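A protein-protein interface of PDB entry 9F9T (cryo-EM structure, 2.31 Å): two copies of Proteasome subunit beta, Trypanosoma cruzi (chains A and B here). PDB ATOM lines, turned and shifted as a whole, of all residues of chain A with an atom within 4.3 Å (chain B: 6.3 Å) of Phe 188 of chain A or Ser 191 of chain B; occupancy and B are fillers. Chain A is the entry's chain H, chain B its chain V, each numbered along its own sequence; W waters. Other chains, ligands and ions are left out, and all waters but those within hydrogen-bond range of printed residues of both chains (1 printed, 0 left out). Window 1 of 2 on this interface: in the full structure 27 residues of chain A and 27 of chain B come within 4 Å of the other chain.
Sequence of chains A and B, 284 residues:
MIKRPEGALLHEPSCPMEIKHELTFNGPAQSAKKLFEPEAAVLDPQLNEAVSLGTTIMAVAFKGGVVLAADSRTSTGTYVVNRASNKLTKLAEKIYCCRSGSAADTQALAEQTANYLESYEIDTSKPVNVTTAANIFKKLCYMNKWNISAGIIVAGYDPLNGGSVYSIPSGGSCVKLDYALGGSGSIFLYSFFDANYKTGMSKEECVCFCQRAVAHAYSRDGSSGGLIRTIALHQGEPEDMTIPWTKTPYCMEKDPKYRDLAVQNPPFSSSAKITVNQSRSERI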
ATOM      1  N   GLY A 185       7.753 -25.406  -8.312  1.00  0.00           N
ATOM      2  CA  GLY A 185       6.462 -25.260  -8.961  1.00  0.00           C
ATOM      3  C   GLY A 185       6.087 -26.494  -9.752  1.00  0.00           C
ATOM      4  O   GLY A 185       4.953 -26.569 -10.167  1.00  0.00           O
ATOM      5  N   SER A 186       6.975 -27.480  -9.870  1.00  0.00           N
ATOM      6  CA  SER A 186       6.713 -28.654 -10.682  1.00  0.00           C
ATOM      7  C   SER A 186       5.540 -29.481 -10.198  1.00  0.00           C
ATOM      8  O   SER A 186       4.798 -29.939 -11.004  1.00  0.00           O
ATOM      9  CB  SER A 186       7.926 -29.573 -10.840  1.00  0.00           C
ATOM     10  OG  SER A 186       8.566 -29.976  -9.626  1.00  0.00           O
ATOM     11  N   ILE A 187       5.354 -29.583  -8.892  1.00  0.00           N
ATOM     12  CA  ILE A 187       4.359 -30.440  -8.261  1.00  0.00           C
ATOM     13  C   ILE A 187       2.937 -29.986  -8.602  1.00  0.00           C
ATOM     14  O   ILE A 187       2.014 -30.772  -8.440  1.00  0.00           O
ATOM     15  CB  ILE A 187       4.606 -30.464  -6.727  1.00  0.00           C
ATOM     16  CG1 ILE A 187       3.854 -31.584  -6.003  1.00  0.00           C
ATOM     17  CG2 ILE A 187       4.220 -29.142  -6.127  1.00  0.00           C
ATOM     18  CD1 ILE A 187       4.584 -32.922  -5.958  1.00  0.00           C
ATOM     19  N   PHE A 188       2.746 -28.760  -9.102  1.00  0.00           N
ATOM     20  CA  PHE A 188       1.462 -28.329  -9.637  1.00  0.00           C
ATOM     21  C   PHE A 188       1.238 -28.698 -11.091  1.00  0.00           C
ATOM     22  O   PHE A 188       0.151 -28.487 -11.580  1.00  0.00           O
ATOM     23  CB  PHE A 188       1.353 -26.801  -9.609  1.00  0.00           C
ATOM     24  CG  PHE A 188       1.372 -26.246  -8.209  1.00  0.00           C
ATOM     25  CD1 PHE A 188       0.355 -26.544  -7.345  1.00  0.00           C
ATOM     26  CD2 PHE A 188       2.500 -25.647  -7.706  1.00  0.00           C
ATOM     27  CE1 PHE A 188       0.431 -26.156  -6.034  1.00  0.00           C
ATOM     28  CE2 PHE A 188       2.587 -25.256  -6.390  1.00  0.00           C
ATOM     29  CZ  PHE A 188       1.525 -25.474  -5.559  1.00  0.00           C
ATOM     30  N   LEU A 189       2.214 -29.214 -11.821  1.00  0.00           N
ATOM     31  CA  LEU A 189       2.065 -29.433 -13.255  1.00  0.00           C
ATOM     32  C   LEU A 189       1.944 -30.886 -13.710  1.00  0.00           C
ATOM     33  O   LEU A 189       1.546 -31.119 -14.826  1.00  0.00           O
ATOM     34  CB  LEU A 189       3.324 -28.827 -13.853  1.00  0.00           C
ATOM     35  CG  LEU A 189       3.340 -27.295 -13.818  1.00  0.00           C
ATOM     36  CD1 LEU A 189       4.483 -26.730 -14.647  1.00  0.00           C
ATOM     37  CD2 LEU A 189       1.996 -26.816 -14.380  1.00  0.00           C
ATOM     38  N   TYR A 190       2.232 -31.874 -12.849  1.00  0.00           N
ATOM     39  CA  TYR A 190       2.136 -33.302 -13.161  1.00  0.00           C
ATOM     40  C   TYR A 190       0.786 -33.614 -13.764  1.00  0.00           C
ATOM     41  O   TYR A 190       0.737 -34.064 -14.870  1.00  0.00           O
ATOM     42  CB  TYR A 190       2.487 -34.140 -11.927  1.00  0.00           C
ATOM     43  CG  TYR A 190       4.012 -34.175 -11.737  1.00  0.00           C
ATOM     44  CD1 TYR A 190       4.814 -34.767 -12.690  1.00  0.00           C
ATOM     45  CD2 TYR A 190       4.661 -33.526 -10.701  1.00  0.00           C
ATOM     46  CE1 TYR A 190       6.189 -34.823 -12.585  1.00  0.00           C
ATOM     47  CE2 TYR A 190       6.066 -33.520 -10.611  1.00  0.00           C
ATOM     48  CZ  TYR A 190       6.842 -34.159 -11.564  1.00  0.00           C
ATOM     49  OH  TYR A 190       8.223 -34.184 -11.556  1.00  0.00           O
ATOM     50  N   HIS A 216       0.338 -21.468 -15.037  1.00  0.00           N
ATOM     51  CA  HIS A 216      -0.446 -22.218 -14.080  1.00  0.00           C
ATOM     52  C   HIS A 216       0.359 -22.518 -12.825  1.00  0.00           C
ATOM     53  O   HIS A 216      -0.105 -22.327 -11.715  1.00  0.00           O
ATOM     54  CB  HIS A 216      -1.040 -23.468 -14.721  1.00  0.00           C
ATOM     55  CG  HIS A 216      -2.355 -23.162 -15.350  1.00  0.00           C
ATOM     56  ND1 HIS A 216      -3.485 -23.036 -14.597  1.00  0.00           N
ATOM     57  CD2 HIS A 216      -2.698 -22.965 -16.602  1.00  0.00           C
ATOM     58  CE1 HIS A 216      -4.482 -22.754 -15.439  1.00  0.00           C
ATOM     59  NE2 HIS A 216      -4.002 -22.692 -16.667  1.00  0.00           N
ATOM     60  N   ALA A 217       1.559 -22.984 -12.985  1.00  0.00           N
ATOM     61  CA  ALA A 217       2.433 -23.201 -11.854  1.00  0.00           C
ATOM     62  C   ALA A 217       2.648 -21.938 -11.044  1.00  0.00           C
ATOM     63  O   ALA A 217       2.435 -21.941  -9.826  1.00  0.00           O
ATOM     64  CB  ALA A 217       3.752 -23.706 -12.357  1.00  0.00           C
ATOM     65  N   ARG A 220       0.101 -20.422  -8.459  1.00  0.00           N
ATOM     66  CA  ARG A 220      -0.237 -21.062  -7.211  1.00  0.00           C
ATOM     67  C   ARG A 220       0.999 -21.234  -6.338  1.00  0.00           C
ATOM     68  O   ARG A 220       0.871 -21.551  -5.164  1.00  0.00           O
ATOM     69  CB  ARG A 220      -0.787 -22.468  -7.473  1.00  0.00           C
ATOM     70  CG  ARG A 220      -2.126 -22.560  -8.182  1.00  0.00           C
ATOM     71  CD  ARG A 220      -3.174 -22.219  -7.117  1.00  0.00           C
ATOM     72  NE  ARG A 220      -4.539 -22.251  -7.548  1.00  0.00           N
ATOM     73  CZ  ARG A 220      -5.578 -22.121  -6.717  1.00  0.00           C
ATOM     74  NH1 ARG A 220      -5.447 -21.878  -5.411  1.00  0.00           N
ATOM     75  NH2 ARG A 220      -6.791 -22.189  -7.232  1.00  0.00           N
ATOM     76  N   ASP A 221       2.192 -21.168  -6.947  1.00  0.00           N
ATOM     77  CA  ASP A 221       3.417 -21.349  -6.196  1.00  0.00           C
ATOM     78  C   ASP A 221       3.898 -19.975  -5.771  1.00  0.00           C
ATOM     79  O   ASP A 221       4.243 -19.184  -6.639  1.00  0.00           O
ATOM     80  CB  ASP A 221       4.462 -22.055  -7.082  1.00  0.00           C
ATOM     81  CG  ASP A 221       5.808 -22.400  -6.443  1.00  0.00           C
ATOM     82  OD1 ASP A 221       5.908 -22.574  -5.192  1.00  0.00           O
ATOM     83  OD2 ASP A 221       6.814 -22.479  -7.219  1.00  0.00           O
ATOM     84  N   ILE B 187      -2.654 -30.938  -3.578  1.00  0.00           N
ATOM     85  CA  ILE B 187      -1.650 -30.082  -4.196  1.00  0.00           C
ATOM     86  C   ILE B 187      -1.451 -30.433  -5.673  1.00  0.00           C
ATOM     87  O   ILE B 187      -0.912 -29.616  -6.405  1.00  0.00           O
ATOM     88  CB  ILE B 187      -0.323 -30.190  -3.394  1.00  0.00           C
ATOM     89  CG1 ILE B 187       0.689 -29.092  -3.731  1.00  0.00           C
ATOM     90  CG2 ILE B 187       0.308 -31.533  -3.629  1.00  0.00           C
ATOM     91  CD1 ILE B 187       0.524 -27.802  -2.934  1.00  0.00           C
ATOM     92  N   PHE B 188      -1.906 -31.604  -6.131  1.00  0.00           N
ATOM     93  CA  PHE B 188      -1.938 -31.925  -7.552  1.00  0.00           C
ATOM     94  C   PHE B 188      -3.178 -31.433  -8.273  1.00  0.00           C
ATOM     95  O   PHE B 188      -3.232 -31.548  -9.477  1.00  0.00           O
ATOM     96  CB  PHE B 188      -1.950 -33.444  -7.762  1.00  0.00           C
ATOM     97  CG  PHE B 188      -0.693 -34.105  -7.264  1.00  0.00           C
ATOM     98  CD1 PHE B 188       0.507 -33.823  -7.859  1.00  0.00           C
ATOM     99  CD2 PHE B 188      -0.684 -34.801  -6.081  1.00  0.00           C
ATOM    100  CE1 PHE B 188       1.669 -34.315  -7.328  1.00  0.00           C
ATOM    101  CE2 PHE B 188       0.479 -35.297  -5.540  1.00  0.00           C
ATOM    102  CZ  PHE B 188       1.660 -35.089  -6.194  1.00  0.00           C
ATOM    103  N   LEU B 189      -4.195 -30.913  -7.604  1.00  0.00           N
ATOM    104  CA  LEU B 189      -5.453 -30.576  -8.258  1.00  0.00           C
ATOM    105  C   LEU B 189      -5.752 -29.088  -8.427  1.00  0.00           C
ATOM    106  O   LEU B 189      -6.620 -28.747  -9.194  1.00  0.00           O
ATOM    107  CB  LEU B 189      -6.512 -31.199  -7.366  1.00  0.00           C
ATOM    108  CG  LEU B 189      -6.566 -32.727  -7.458  1.00  0.00           C
ATOM    109  CD1 LEU B 189      -7.794 -33.285  -6.754  1.00  0.00           C
ATOM    110  CD2 LEU B 189      -6.603 -33.090  -8.946  1.00  0.00           C
ATOM    111  N   TYR B 190      -5.011 -28.187  -7.763  1.00  0.00           N
ATOM    112  CA  TYR B 190      -5.188 -26.734  -7.857  1.00  0.00           C
ATOM    113  C   TYR B 190      -5.221 -26.307  -9.306  1.00  0.00           C
ATOM    114  O   TYR B 190      -6.201 -25.771  -9.730  1.00  0.00           O
ATOM    115  CB  TYR B 190      -4.137 -26.015  -7.007  1.00  0.00           C
ATOM    116  CG  TYR B 190      -4.537 -26.074  -5.523  1.00  0.00           C
ATOM    117  CD1 TYR B 190      -5.692 -25.452  -5.091  1.00  0.00           C
ATOM    118  CD2 TYR B 190      -3.859 -26.835  -4.587  1.00  0.00           C
ATOM    119  CE1 TYR B 190      -6.111 -25.477  -3.777  1.00  0.00           C
ATOM    120  CE2 TYR B 190      -4.310 -26.922  -3.255  1.00  0.00           C
ATOM    121  CZ  TYR B 190      -5.449 -26.250  -2.843  1.00  0.00           C
ATOM    122  OH  TYR B 190      -5.964 -26.303  -1.560  1.00  0.00           O
ATOM    123  N   SER B 191      -4.168 -26.640 -10.035  1.00  0.00           N
ATOM    124  CA  SER B 191      -3.976 -26.376 -11.449  1.00  0.00           C
ATOM    125  C   SER B 191      -4.997 -27.091 -12.327  1.00  0.00           C
ATOM    126  O   SER B 191      -5.455 -26.545 -13.293  1.00  0.00           O
ATOM    127  CB  SER B 191      -2.556 -26.726 -11.861  1.00  0.00           C
ATOM    128  OG  SER B 191      -1.619 -25.811 -11.278  1.00  0.00           O
ATOM    129  N   PHE B 192      -5.396 -28.270 -11.938  1.00  0.00           N
ATOM    130  CA  PHE B 192      -6.420 -29.021 -12.630  1.00  0.00           C
ATOM    131  C   PHE B 192      -7.669 -28.179 -12.651  1.00  0.00           C
ATOM    132  O   PHE B 192      -8.246 -27.941 -13.678  1.00  0.00           O
ATOM    133  CB  PHE B 192      -6.675 -30.351 -11.863  1.00  0.00           C
ATOM    134  CG  PHE B 192      -7.477 -31.328 -12.665  1.00  0.00           C
ATOM    135  CD1 PHE B 192      -6.974 -31.790 -13.863  1.00  0.00           C
ATOM    136  CD2 PHE B 192      -8.778 -31.587 -12.337  1.00  0.00           C
ATOM    137  CE1 PHE B 192      -7.767 -32.528 -14.724  1.00  0.00           C
ATOM    138  CE2 PHE B 192      -9.574 -32.354 -13.183  1.00  0.00           C
ATOM    139  CZ  PHE B 192      -9.086 -32.781 -14.402  1.00  0.00           C
ATOM    140  N   PHE B 193      -8.127 -27.803 -11.469  1.00  0.00           N
ATOM    141  CA  PHE B 193      -9.319 -26.995 -11.286  1.00  0.00           C
ATOM    142  C   PHE B 193      -9.228 -25.617 -11.910  1.00  0.00           C
ATOM    143  O   PHE B 193     -10.167 -25.178 -12.519  1.00  0.00           O
ATOM    144  CB  PHE B 193      -9.521 -26.727  -9.799  1.00  0.00           C
ATOM    145  CG  PHE B 193     -10.395 -27.758  -9.193  1.00  0.00           C
ATOM    146  CD1 PHE B 193      -9.969 -29.051  -9.145  1.00  0.00           C
ATOM    147  CD2 PHE B 193     -11.689 -27.454  -8.819  1.00  0.00           C
ATOM    148  CE1 PHE B 193     -10.746 -30.042  -8.583  1.00  0.00           C
ATOM    149  CE2 PHE B 193     -12.503 -28.462  -8.317  1.00  0.00           C
ATOM    150  CZ  PHE B 193     -12.009 -29.760  -8.180  1.00  0.00           C
ATOM    151  N   ASP B 194      -8.114 -24.933 -11.740  1.00  0.00           N
ATOM    152  CA  ASP B 194      -7.869 -23.663 -12.415  1.00  0.00           C
ATOM    153  C   ASP B 194      -8.032 -23.733 -13.943  1.00  0.00           C
ATOM    154  O   ASP B 194      -8.542 -22.818 -14.557  1.00  0.00           O
ATOM    155  CB  ASP B 194      -6.474 -23.155 -12.045  1.00  0.00           C
ATOM    156  CG  ASP B 194      -6.371 -22.678 -10.590  1.00  0.00           C
ATOM    157  OD1 ASP B 194      -7.436 -22.677  -9.914  1.00  0.00           O
ATOM    158  OD2 ASP B 194      -5.172 -22.356 -10.130  1.00  0.00           O
ATOM    159  N   ALA B 195      -7.563 -24.811 -14.521  1.00  0.00           N
ATOM    160  CA  ALA B 195      -7.529 -25.076 -15.953  1.00  0.00           C
ATOM    161  C   ALA B 195      -8.834 -25.658 -16.506  1.00  0.00           C
ATOM    162  O   ALA B 195      -9.235 -25.309 -17.602  1.00  0.00           O
ATOM    163  CB  ALA B 195      -6.387 -26.013 -16.197  1.00  0.00           C
ATOM    164  N   ASN B 196      -9.577 -26.444 -15.729  1.00  0.00           N
ATOM    165  CA  ASN B 196     -10.590 -27.358 -16.265  1.00  0.00           C
ATOM    166  C   ASN B 196     -11.948 -27.200 -15.592  1.00  0.00           C
ATOM    167  O   ASN B 196     -12.920 -27.736 -16.113  1.00  0.00           O
ATOM    168  CB  ASN B 196     -10.190 -28.830 -16.067  1.00  0.00           C
ATOM    169  CG  ASN B 196      -8.935 -29.198 -16.833  1.00  0.00           C
ATOM    170  OD1 ASN B 196      -8.097 -29.950 -16.359  1.00  0.00           O
ATOM    171  ND2 ASN B 196      -8.794 -28.680 -18.037  1.00  0.00           N
HETATM  172  O   HOH W   1      -2.772 -22.913 -11.738  1.00  0.00           O
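Hydrophobic or aromatic side chains of chain B that line the printed part of chain A: Ile 187, Phe 188, Tyr 190 and Ala 195.
Hydrophobic or aromatic side chains of chain A within 4 Å of the printed part of chain B: Ile 187, Phe 188 and His 216.
Among the printed residues, 9 pairs touch across the chains.
Among the printed residues, Asp or Glu carboxylates within 4 Å of a Lys or Arg side-chain nitrogen of the other chain: Arg 220 of chain A with Asp 194 of chain B (2.7 Å).
OD2 of Asp 194 of chain B lies within salt-bridge range of NE of Arg 220 of chain A (2.7 Å).
O of Phe 188 of chain A lies within hydrogen-bond range of OG of Ser 191 of chain B, at 3.2 Å.
Ile 187 of chain B touches its own counterpart, Ile 187 of chain A.
Ile 187 of chain A touches Phe 188 of chain B, and with the chains exchanged Phe 188 of chain A touches Ile 187 of chain B.
Of the 9 pairs that touch across the chains among the printed residues, 3 have their exchanged pair printed and touching as well.
Of chain B, only Ile 187 (3.5 Å) and Ser 191 (3.2 Å) come within 4 Å of Phe 188 of chain A.
Ser 191 of chain B touches just these residues of chain A: Phe 188 (3.2 Å) and His 216 (3.8 Å).
Of the printed residues of chain A, Tyr 190 of chain B touches Arg 220.
Printed residues of chain A within 4 Å of Ile 187 of chain B: Ile 187 and Phe 188.
Printed residues of chain B within 4 Å of Arg 220 of chain A: Tyr 190 (3.6 Å) and Asp 194 (2.7 Å).
Printed residues of chain A within 4 Å of Phe 188 of chain B: Ile 187.
Asp 221 of chain A touches none of the printed residues of chain B.
Phe 193 of chain B touches none of the printed residues of chain A.
The nearest residue of chain B that does not touch Phe 188 of chain A is Tyr 190 of chain B (4.5 Å).
Water W1 lies within hydrogen-bond range of O of His 216 of chain A (2.7 Å), OD2 of Asp 194 of chain B (2.9 Å) and OG of Ser 191 of chain B (3.2 Å).
O of Ile 187 of chain A touches O of Ile 187 of chain B, at 3.7 Å.
Phe 188 of chain B touches Ile 187 of chain A.
CD1 of Phe 188 of chain A touches O of Ile 187 of chain B, 3.5 Å away.
Ser 191 of chain B touches His 216 of chain A (OG to O, 3.8 Å).
His 216 of chain A touches Asp 194 of chain B (ND1 to CB, 3.9 Å).
CE1 of His 216 of chain A touches N of Ala 195 of chain B, 3.8 Å away.
Arg 220 of chain A touches Tyr 190 of chain B (NH1 to CD1, 3.6 Å).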
